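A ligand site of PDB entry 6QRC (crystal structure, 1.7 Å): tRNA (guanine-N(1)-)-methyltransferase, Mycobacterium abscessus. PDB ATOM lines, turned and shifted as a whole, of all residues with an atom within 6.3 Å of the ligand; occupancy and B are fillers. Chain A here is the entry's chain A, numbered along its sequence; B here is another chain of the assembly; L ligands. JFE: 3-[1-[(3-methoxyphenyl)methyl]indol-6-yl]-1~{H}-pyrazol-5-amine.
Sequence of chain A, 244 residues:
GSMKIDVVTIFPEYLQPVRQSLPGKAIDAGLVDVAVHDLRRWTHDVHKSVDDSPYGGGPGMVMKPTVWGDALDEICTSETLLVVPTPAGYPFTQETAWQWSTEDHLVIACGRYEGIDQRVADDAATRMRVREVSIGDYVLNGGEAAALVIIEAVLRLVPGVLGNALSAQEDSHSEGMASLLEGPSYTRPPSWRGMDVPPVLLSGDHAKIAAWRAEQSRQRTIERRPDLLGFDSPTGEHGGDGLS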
ATOM      1  N   PRO A  85      -5.079  13.753  -9.259  1.00  0.00           N
ATOM      2  CA  PRO A  85      -4.816  13.444  -7.847  1.00  0.00           C
ATOM      3  C   PRO A  85      -3.549  12.632  -7.672  1.00  0.00           C
ATOM      4  O   PRO A  85      -3.275  11.755  -8.479  1.00  0.00           O
ATOM      5  CB  PRO A  85      -6.042  12.644  -7.413  1.00  0.00           C
ATOM      6  CG  PRO A  85      -7.151  13.142  -8.331  1.00  0.00           C
ATOM      7  CD  PRO A  85      -6.435  13.334  -9.661  1.00  0.00           C
ATOM      8  N   THR A  86      -2.809  12.919  -6.614  1.00  0.00           N
ATOM      9  CA  THR A  86      -1.577  12.180  -6.342  1.00  0.00           C
ATOM     10  C   THR A  86      -1.084  12.533  -4.955  1.00  0.00           C
ATOM     11  O   THR A  86      -1.188  13.676  -4.555  1.00  0.00           O
ATOM     12  CB  THR A  86      -0.445  12.458  -7.393  1.00  0.00           C
ATOM     13  OG1 THR A  86       0.822  12.028  -6.870  1.00  0.00           O
ATOM     14  CG2 THR A  86      -0.349  13.936  -7.790  1.00  0.00           C
ATOM     15  N   PRO A  87      -0.544  11.552  -4.223  1.00  0.00           N
ATOM     16  CA  PRO A  87      -0.009  11.897  -2.878  1.00  0.00           C
ATOM     17  C   PRO A  87       1.139  12.884  -2.954  1.00  0.00           C
ATOM     18  O   PRO A  87       1.485  13.507  -1.930  1.00  0.00           O
ATOM     19  CB  PRO A  87       0.486  10.555  -2.327  1.00  0.00           C
ATOM     20  CG  PRO A  87      -0.039   9.514  -3.223  1.00  0.00           C
ATOM     21  CD  PRO A  87      -0.309  10.148  -4.569  1.00  0.00           C
ATOM     22  N   ALA A  88       1.747  13.006  -4.130  1.00  0.00           N
ATOM     23  CA  ALA A  88       2.877  13.898  -4.347  1.00  0.00           C
ATOM     24  C   ALA A  88       2.450  15.254  -4.910  1.00  0.00           C
ATOM     25  O   ALA A  88       3.284  16.033  -5.379  1.00  0.00           O
ATOM     26  CB  ALA A  88       3.912  13.239  -5.284  1.00  0.00           C
ATOM     27  N   CYS A 110      -7.923   9.832 -12.722  1.00  0.00           N
ATOM     28  CA  CYS A 110      -7.724   9.001 -11.540  1.00  0.00           C
ATOM     29  C   CYS A 110      -6.772   7.857 -11.800  1.00  0.00           C
ATOM     30  O   CYS A 110      -7.056   6.958 -12.597  1.00  0.00           O
ATOM     31  CB  CYS A 110      -9.052   8.426 -11.062  1.00  0.00           C
ATOM     32  SG  CYS A 110     -10.288   9.673 -10.665  1.00  0.00           S
ATOM     33  N   GLY A 111      -5.642   7.876 -11.111  1.00  0.00           N
ATOM     34  CA  GLY A 111      -4.693   6.804 -11.208  1.00  0.00           C
ATOM     35  C   GLY A 111      -5.025   5.681 -10.250  1.00  0.00           C
ATOM     36  O   GLY A 111      -5.833   5.825  -9.336  1.00  0.00           O
ATOM     37  N   ARG A 112      -4.377   4.537 -10.491  1.00  0.00           N
ATOM     38  CA  ARG A 112      -4.356   3.411  -9.566  1.00  0.00           C
ATOM     39  C   ARG A 112      -2.928   2.868  -9.560  1.00  0.00           C
ATOM     40  O   ARG A 112      -2.013   3.520 -10.083  1.00  0.00           O
ATOM     41  CB  ARG A 112      -5.383   2.344  -9.952  1.00  0.00           C
ATOM     42  CG  ARG A 112      -6.813   2.665  -9.534  1.00  0.00           C
ATOM     43  CD  ARG A 112      -7.132   2.112  -8.142  1.00  0.00           C
ATOM     44  NE  ARG A 112      -8.233   2.820  -7.511  1.00  0.00           N
ATOM     45  CZ  ARG A 112      -8.793   2.442  -6.366  1.00  0.00           C
ATOM     46  NH1 ARG A 112      -8.367   1.334  -5.762  1.00  0.00           N
ATOM     47  NH2 ARG A 112      -9.800   3.141  -5.844  1.00  0.00           N
ATOM     48  N   TYR A 113      -2.738   1.689  -8.968  1.00  0.00           N
ATOM     49  CA  TYR A 113      -1.399   1.119  -8.824  1.00  0.00           C
ATOM     50  C   TYR A 113      -0.485   2.123  -8.133  1.00  0.00           C
ATOM     51  O   TYR A 113      -0.827   2.654  -7.076  1.00  0.00           O
ATOM     52  CB  TYR A 113      -0.843   0.677 -10.189  1.00  0.00           C
ATOM     53  CG  TYR A 113      -1.805  -0.225 -10.936  1.00  0.00           C
ATOM     54  CD1 TYR A 113      -1.728  -1.608 -10.805  1.00  0.00           C
ATOM     55  CD2 TYR A 113      -2.791   0.301 -11.756  1.00  0.00           C
ATOM     56  CE1 TYR A 113      -2.613  -2.443 -11.474  1.00  0.00           C
ATOM     57  CE2 TYR A 113      -3.681  -0.516 -12.428  1.00  0.00           C
ATOM     58  CZ  TYR A 113      -3.589  -1.891 -12.281  1.00  0.00           C
ATOM     59  OH  TYR A 113      -4.479  -2.708 -12.954  1.00  0.00           O
ATOM     60  N   GLU A 114       0.675   2.384  -8.717  1.00  0.00           N
ATOM     61  CA  GLU A 114       1.619   3.351  -8.153  1.00  0.00           C
ATOM     62  C   GLU A 114       1.598   4.692  -8.888  1.00  0.00           C
ATOM     63  O   GLU A 114       2.492   5.503  -8.729  1.00  0.00           O
ATOM     64  CB  GLU A 114       3.046   2.799  -8.187  1.00  0.00           C
ATOM     65  CG  GLU A 114       3.228   1.505  -7.423  1.00  0.00           C
ATOM     66  CD  GLU A 114       3.248   1.717  -5.932  1.00  0.00           C
ATOM     67  OE1 GLU A 114       2.171   1.654  -5.307  1.00  0.00           O
ATOM     68  OE2 GLU A 114       4.351   1.963  -5.392  1.00  0.00           O
ATOM     69  N   GLY A 115       0.565   4.902  -9.707  1.00  0.00           N
ATOM     70  CA  GLY A 115       0.402   6.182 -10.355  1.00  0.00           C
ATOM     71  C   GLY A 115       0.538   6.130 -11.867  1.00  0.00           C
ATOM     72  O   GLY A 115       0.603   5.057 -12.447  1.00  0.00           O
ATOM     73  N   ILE A 116       0.586   7.301 -12.491  1.00  0.00           N
ATOM     74  CA  ILE A 116       0.581   7.414 -13.944  1.00  0.00           C
ATOM     75  C   ILE A 116       1.959   7.833 -14.426  1.00  0.00           C
ATOM     76  O   ILE A 116       2.578   8.715 -13.825  1.00  0.00           O
ATOM     77  CB  ILE A 116      -0.459   8.447 -14.412  1.00  0.00           C
ATOM     78  CG1 ILE A 116      -1.836   8.077 -13.836  1.00  0.00           C
ATOM     79  CG2 ILE A 116      -0.470   8.551 -15.957  1.00  0.00           C
ATOM     80  CD1 ILE A 116      -2.896   9.152 -14.010  1.00  0.00           C
ATOM     81  N   VAL A 133      -2.524  17.336  -7.629  1.00  0.00           N
ATOM     82  CA  VAL A 133      -2.901  17.756  -6.286  1.00  0.00           C
ATOM     83  C   VAL A 133      -3.075  16.624  -5.306  1.00  0.00           C
ATOM     84  O   VAL A 133      -3.495  15.532  -5.682  1.00  0.00           O
ATOM     85  CB  VAL A 133      -4.223  18.576  -6.299  1.00  0.00           C
ATOM     86  CG1 VAL A 133      -4.015  19.914  -7.022  1.00  0.00           C
ATOM     87  CG2 VAL A 133      -5.367  17.772  -6.957  1.00  0.00           C
ATOM     88  N   SER A 134      -2.759  16.908  -4.045  1.00  0.00           N
ATOM     89  CA  SER A 134      -3.004  15.994  -2.931  1.00  0.00           C
ATOM     90  C   SER A 134      -4.183  16.502  -2.097  1.00  0.00           C
ATOM     91  O   SER A 134      -4.283  17.706  -1.874  1.00  0.00           O
ATOM     92  CB  SER A 134      -1.757  15.892  -2.050  1.00  0.00           C
ATOM     93  OG  SER A 134      -2.037  15.219  -0.841  1.00  0.00           O
ATOM     94  N   ILE A 135      -5.045  15.614  -1.612  1.00  0.00           N
ATOM     95  CA  ILE A 135      -6.170  16.086  -0.762  1.00  0.00           C
ATOM     96  C   ILE A 135      -5.882  15.958   0.735  1.00  0.00           C
ATOM     97  O   ILE A 135      -6.736  16.327   1.570  1.00  0.00           O
ATOM     98  CB  ILE A 135      -7.501  15.357  -1.067  1.00  0.00           C
ATOM     99  CG1 ILE A 135      -7.386  13.848  -0.827  1.00  0.00           C
ATOM    100  CG2 ILE A 135      -7.978  15.703  -2.494  1.00  0.00           C
ATOM    101  CD1 ILE A 135      -8.755  13.167  -0.567  1.00  0.00           C
ATOM    102  N   GLY A 136      -4.705  15.460   1.076  1.00  0.00           N
ATOM    103  CA  GLY A 136      -4.331  15.346   2.481  1.00  0.00           C
ATOM    104  C   GLY A 136      -3.114  14.470   2.666  1.00  0.00           C
ATOM    105  O   GLY A 136      -2.689  13.775   1.736  1.00  0.00           O
ATOM    106  N   ASP A 137      -2.542  14.480   3.865  1.00  0.00           N
ATOM    107  CA  ASP A 137      -1.291  13.743   4.067  1.00  0.00           C
ATOM    108  C   ASP A 137      -1.521  12.301   4.502  1.00  0.00           C
ATOM    109  O   ASP A 137      -1.120  11.879   5.585  1.00  0.00           O
ATOM    110  CB  ASP A 137      -0.408  14.486   5.071  1.00  0.00           C
ATOM    111  CG  ASP A 137       0.106  15.785   4.509  1.00  0.00           C
ATOM    112  OD1 ASP A 137       0.353  15.830   3.294  1.00  0.00           O
ATOM    113  OD2 ASP A 137       0.255  16.769   5.268  1.00  0.00           O
ATOM    114  N   TYR A 138      -2.177  11.546   3.631  1.00  0.00           N
ATOM    115  CA  TYR A 138      -2.398  10.130   3.811  1.00  0.00           C
ATOM    116  C   TYR A 138      -2.366   9.542   2.427  1.00  0.00           C
ATOM    117  O   TYR A 138      -2.493  10.261   1.436  1.00  0.00           O
ATOM    118  CB  TYR A 138      -3.736   9.832   4.485  1.00  0.00           C
ATOM    119  CG  TYR A 138      -4.798  10.795   4.010  1.00  0.00           C
ATOM    120  CD1 TYR A 138      -5.405  10.620   2.768  1.00  0.00           C
ATOM    121  CD2 TYR A 138      -5.167  11.881   4.777  1.00  0.00           C
ATOM    122  CE1 TYR A 138      -6.342  11.512   2.309  1.00  0.00           C
ATOM    123  CE2 TYR A 138      -6.127  12.789   4.321  1.00  0.00           C
ATOM    124  CZ  TYR A 138      -6.699  12.591   3.075  1.00  0.00           C
ATOM    125  OH  TYR A 138      -7.638  13.480   2.607  1.00  0.00           O
ATOM    126  N   VAL A 139      -2.228   8.231   2.361  1.00  0.00           N
ATOM    127  CA  VAL A 139      -2.109   7.567   1.069  1.00  0.00           C
ATOM    128  C   VAL A 139      -3.357   6.768   0.781  1.00  0.00           C
ATOM    129  O   VAL A 139      -3.770   5.954   1.603  1.00  0.00           O
ATOM    130  CB  VAL A 139      -0.878   6.630   1.030  1.00  0.00           C
ATOM    131  CG1 VAL A 139      -0.783   5.956  -0.339  1.00  0.00           C
ATOM    132  CG2 VAL A 139       0.382   7.406   1.343  1.00  0.00           C
ATOM    133  N   LEU A 140      -3.975   7.004  -0.385  1.00  0.00           N
ATOM    134  CA  LEU A 140      -5.118   6.231  -0.828  1.00  0.00           C
ATOM    135  C   LEU A 140      -4.678   5.099  -1.763  1.00  0.00           C
ATOM    136  O   LEU A 140      -3.502   4.996  -2.083  1.00  0.00           O
ATOM    137  CB  LEU A 140      -6.122   7.127  -1.558  1.00  0.00           C
ATOM    138  CG  LEU A 140      -6.636   8.334  -0.740  1.00  0.00           C
ATOM    139  CD1 LEU A 140      -7.256   9.363  -1.655  1.00  0.00           C
ATOM    140  CD2 LEU A 140      -7.628   7.871   0.311  1.00  0.00           C
ATOM    141  N   ASN A 141      -5.618   4.273  -2.205  1.00  0.00           N
ATOM    142  CA  ASN A 141      -5.266   3.246  -3.187  1.00  0.00           C
ATOM    143  C   ASN A 141      -5.300   3.774  -4.624  1.00  0.00           C
ATOM    144  O   ASN A 141      -4.760   3.151  -5.551  1.00  0.00           O
ATOM    145  CB  ASN A 141      -6.218   2.050  -3.088  1.00  0.00           C
ATOM    146  CG  ASN A 141      -5.804   1.072  -2.022  1.00  0.00           C
ATOM    147  OD1 ASN A 141      -4.608   0.928  -1.715  1.00  0.00           O
ATOM    148  ND2 ASN A 141      -6.770   0.374  -1.452  1.00  0.00           N
ATOM    149  N   GLY A 142      -5.930   4.921  -4.818  1.00  0.00           N
ATOM    150  CA  GLY A 142      -6.042   5.484  -6.146  1.00  0.00           C
ATOM    151  C   GLY A 142      -6.725   6.822  -6.098  1.00  0.00           C
ATOM    152  O   GLY A 142      -7.050   7.310  -5.013  1.00  0.00           O
ATOM    153  N   GLY A 143      -6.944   7.430  -7.270  1.00  0.00           N
ATOM    154  CA  GLY A 143      -7.410   8.803  -7.323  1.00  0.00           C
ATOM    155  C   GLY A 143      -8.900   9.016  -7.116  1.00  0.00           C
ATOM    156  O   GLY A 143      -9.340  10.152  -6.964  1.00  0.00           O
ATOM    157  N   GLU A 144      -9.674   7.921  -7.104  1.00  0.00           N
ATOM    158  CA  GLU A 144     -11.127   8.061  -7.156  1.00  0.00           C
ATOM    159  C   GLU A 144     -11.714   8.733  -5.919  1.00  0.00           C
ATOM    160  O   GLU A 144     -12.579   9.605  -6.039  1.00  0.00           O
ATOM    161  CB  GLU A 144     -11.793   6.695  -7.327  1.00  0.00           C
ATOM    162  CG  GLU A 144     -11.613   6.101  -8.719  1.00  0.00           C
ATOM    163  CD  GLU A 144     -10.256   5.445  -8.932  1.00  0.00           C
ATOM    164  OE1 GLU A 144      -9.479   5.263  -7.963  1.00  0.00           O
ATOM    165  OE2 GLU A 144      -9.966   5.070 -10.091  1.00  0.00           O
ATOM    166  N   ALA A 146     -10.256  10.785  -4.007  1.00  0.00           N
ATOM    167  CA  ALA A 146      -9.811  12.167  -4.111  1.00  0.00           C
ATOM    168  C   ALA A 146     -10.692  12.928  -5.097  1.00  0.00           C
ATOM    169  O   ALA A 146     -11.034  14.073  -4.867  1.00  0.00           O
ATOM    170  CB  ALA A 146      -8.347  12.243  -4.526  1.00  0.00           C
ATOM    171  N   ARG B 156      -6.080  -0.196   3.703  1.00  0.00           N
ATOM    172  CA  ARG B 156      -4.896  -0.633   2.955  1.00  0.00           C
ATOM    173  C   ARG B 156      -3.677  -0.884   3.862  1.00  0.00           C
ATOM    174  O   ARG B 156      -2.646  -1.406   3.415  1.00  0.00           O
ATOM    175  CB  ARG B 156      -4.556   0.382   1.863  1.00  0.00           C
ATOM    176  CG  ARG B 156      -4.052   1.709   2.368  1.00  0.00           C
ATOM    177  CD  ARG B 156      -3.948   2.697   1.221  1.00  0.00           C
ATOM    178  NE  ARG B 156      -2.870   2.386   0.287  1.00  0.00           N
ATOM    179  CZ  ARG B 156      -1.574   2.582   0.540  1.00  0.00           C
ATOM    180  NH1 ARG B 156      -1.177   3.079   1.712  1.00  0.00           N
ATOM    181  NH2 ARG B 156      -0.675   2.269  -0.387  1.00  0.00           N
ATOM    182  N   GLU B 182       6.741  11.287  -3.172  1.00  0.00           N
ATOM    183  CA  GLU B 182       7.077  10.365  -4.241  1.00  0.00           C
ATOM    184  C   GLU B 182       7.512  11.111  -5.491  1.00  0.00           C
ATOM    185  O   GLU B 182       6.871  12.085  -5.915  1.00  0.00           O
ATOM    186  CB  GLU B 182       5.877   9.477  -4.562  1.00  0.00           C
ATOM    187  CG  GLU B 182       5.682   8.327  -3.593  1.00  0.00           C
ATOM    188  CD  GLU B 182       6.600   7.175  -3.895  1.00  0.00           C
ATOM    189  OE1 GLU B 182       7.757   7.192  -3.417  1.00  0.00           O
ATOM    190  OE2 GLU B 182       6.185   6.264  -4.642  1.00  0.00           O
ATOM    191  N   GLY B 183       8.622  10.666  -6.077  1.00  0.00           N
ATOM    192  CA  GLY B 183       9.094  11.200  -7.335  1.00  0.00           C
ATOM    193  C   GLY B 183       8.304  10.635  -8.509  1.00  0.00           C
ATOM    194  O   GLY B 183       7.378   9.852  -8.323  1.00  0.00           O
HETATM  195  C10 JFE L   1      -3.301   7.576  -6.796  1.00  0.00           C
HETATM  196  C15 JFE L   1      -0.241   5.348  -4.622  1.00  0.00           C
HETATM  197  C17 JFE L   1       1.885   4.965  -3.567  1.00  0.00           C
HETATM  198  C20 JFE L   1       0.331   6.369  -5.394  1.00  0.00           C
HETATM  199  C22 JFE L   1       1.527   8.209  -7.124  1.00  0.00           C
HETATM  200  C24 JFE L   1      -2.984   6.572  -7.775  1.00  0.00           C
HETATM  201  N01 JFE L   1      -3.902  12.841  -1.107  1.00  0.00           N
HETATM  202  C02 JFE L   1      -3.768  11.597  -1.736  1.00  0.00           C
HETATM  203  N03 JFE L   1      -3.542  10.427  -1.092  1.00  0.00           N
HETATM  204  N04 JFE L   1      -3.471   9.427  -2.003  1.00  0.00           N
HETATM  205  C05 JFE L   1      -3.693   9.932  -3.211  1.00  0.00           C
HETATM  206  C06 JFE L   1      -3.851  11.297  -3.111  1.00  0.00           C
HETATM  207  C07 JFE L   1      -3.625   9.111  -4.490  1.00  0.00           C
HETATM  208  C08 JFE L   1      -4.076   9.632  -5.702  1.00  0.00           C
HETATM  209  C09 JFE L   1      -3.905   8.860  -6.863  1.00  0.00           C
HETATM  210  C11 JFE L   1      -2.843   7.079  -5.581  1.00  0.00           C
HETATM  211  C12 JFE L   1      -2.996   7.866  -4.420  1.00  0.00           C
HETATM  212  N13 JFE L   1      -2.298   5.840  -5.800  1.00  0.00           N
HETATM  213  C14 JFE L   1      -1.719   5.006  -4.797  1.00  0.00           C
HETATM  214  C16 JFE L   1       0.528   4.648  -3.717  1.00  0.00           C
HETATM  215  C18 JFE L   1       2.467   5.988  -4.342  1.00  0.00           C
HETATM  216  C19 JFE L   1       1.712   6.683  -5.239  1.00  0.00           C
HETATM  217  O21 JFE L   1       2.297   7.720  -5.997  1.00  0.00           O
HETATM  218  C23 JFE L   1      -2.380   5.520  -7.117  1.00  0.00           C
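O of Tyr 138 is in hydrogen-bond range of N03 of the ligand (2.7 Å).
A nitrogen (N04) of the ligand lies within hydrogen-bond range of the backbone NH (N) of Leu 140 (3.0 Å).
The side-chain hydroxyl (OG) of Ser 134 lies within hydrogen-bond range of a nitrogen (N01) of the ligand.
The backbone carbonyl oxygen (O) of Gly 136 lies within hydrogen-bond range of a nitrogen (N01) of the ligand, at 3.2 Å.
N01 of the ligand sits close to N of Ile 135, 3.0 Å away.
O of Pro 85 touches C09 of the ligand (3.4 Å).
C of Thr 86 touches C06 of the ligand, 3.5 Å away.
Pro 87 touches the ligand.
Gly 111 touches the ligand (C to C24, 3.3 Å).
O of Arg 112 touches C23 of the ligand, at 3.6 Å.
Tyr 113 touches the ligand.
Glu 114 touches the ligand (O to C22, 3.3 Å).
Gly 115 touches the ligand.
Val 139 touches the ligand (CA to N04, 3.8 Å).
Asn 141 touches the ligand (O to C14, 3.6 Å).
Gly 142 touches the ligand.
Gly 143 touches the ligand.
OE2 of Glu 182 of chain B touches C18 of the ligand, at 3.7 Å.
Hydrophobic or aromatic side chains within 4 Å of the ligand: Pro 85, Pro 87, Ile 135, Val 139 and Leu 140.
Of the 27 residues printed, 18 come within 4 Å of the ligand.
Along chain A the residues within 4 Å of the ligand span positions 85 to 143.
The nearest printed residue that does not touch the ligand is Arg 156 of chain B (4.3 Å).
The side-chain hydroxyl of Tyr 138 lies within hydrogen-bond range of the backbone carbonyl oxygen of Ile 135, 3.2 Å away.
O of Gly 136 is in hydrogen-bond range of OG of Ser 134 (3.0 Å).
N of Gly 143 lies within hydrogen-bond range of O of Gly 111 (2.8 Å).
The backbone carbonyl oxygen (O) of Val 133 is in hydrogen-bond range of the backbone NH (N) of Thr 86 (2.9 Å).
The backbone NH (N) of Ala 88 lies close to the side-chain hydroxyl (OG1) of Thr 86 (3.1 Å).
The guanidinium group (NE) of Arg 112 lies within salt-bridge range of the side-chain carboxylate (OE1) of Glu 144 (2.8 Å).
NE of Arg 156 of chain B is in hydrogen-bond range of OD1 of Asn 141 (3.0 Å).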
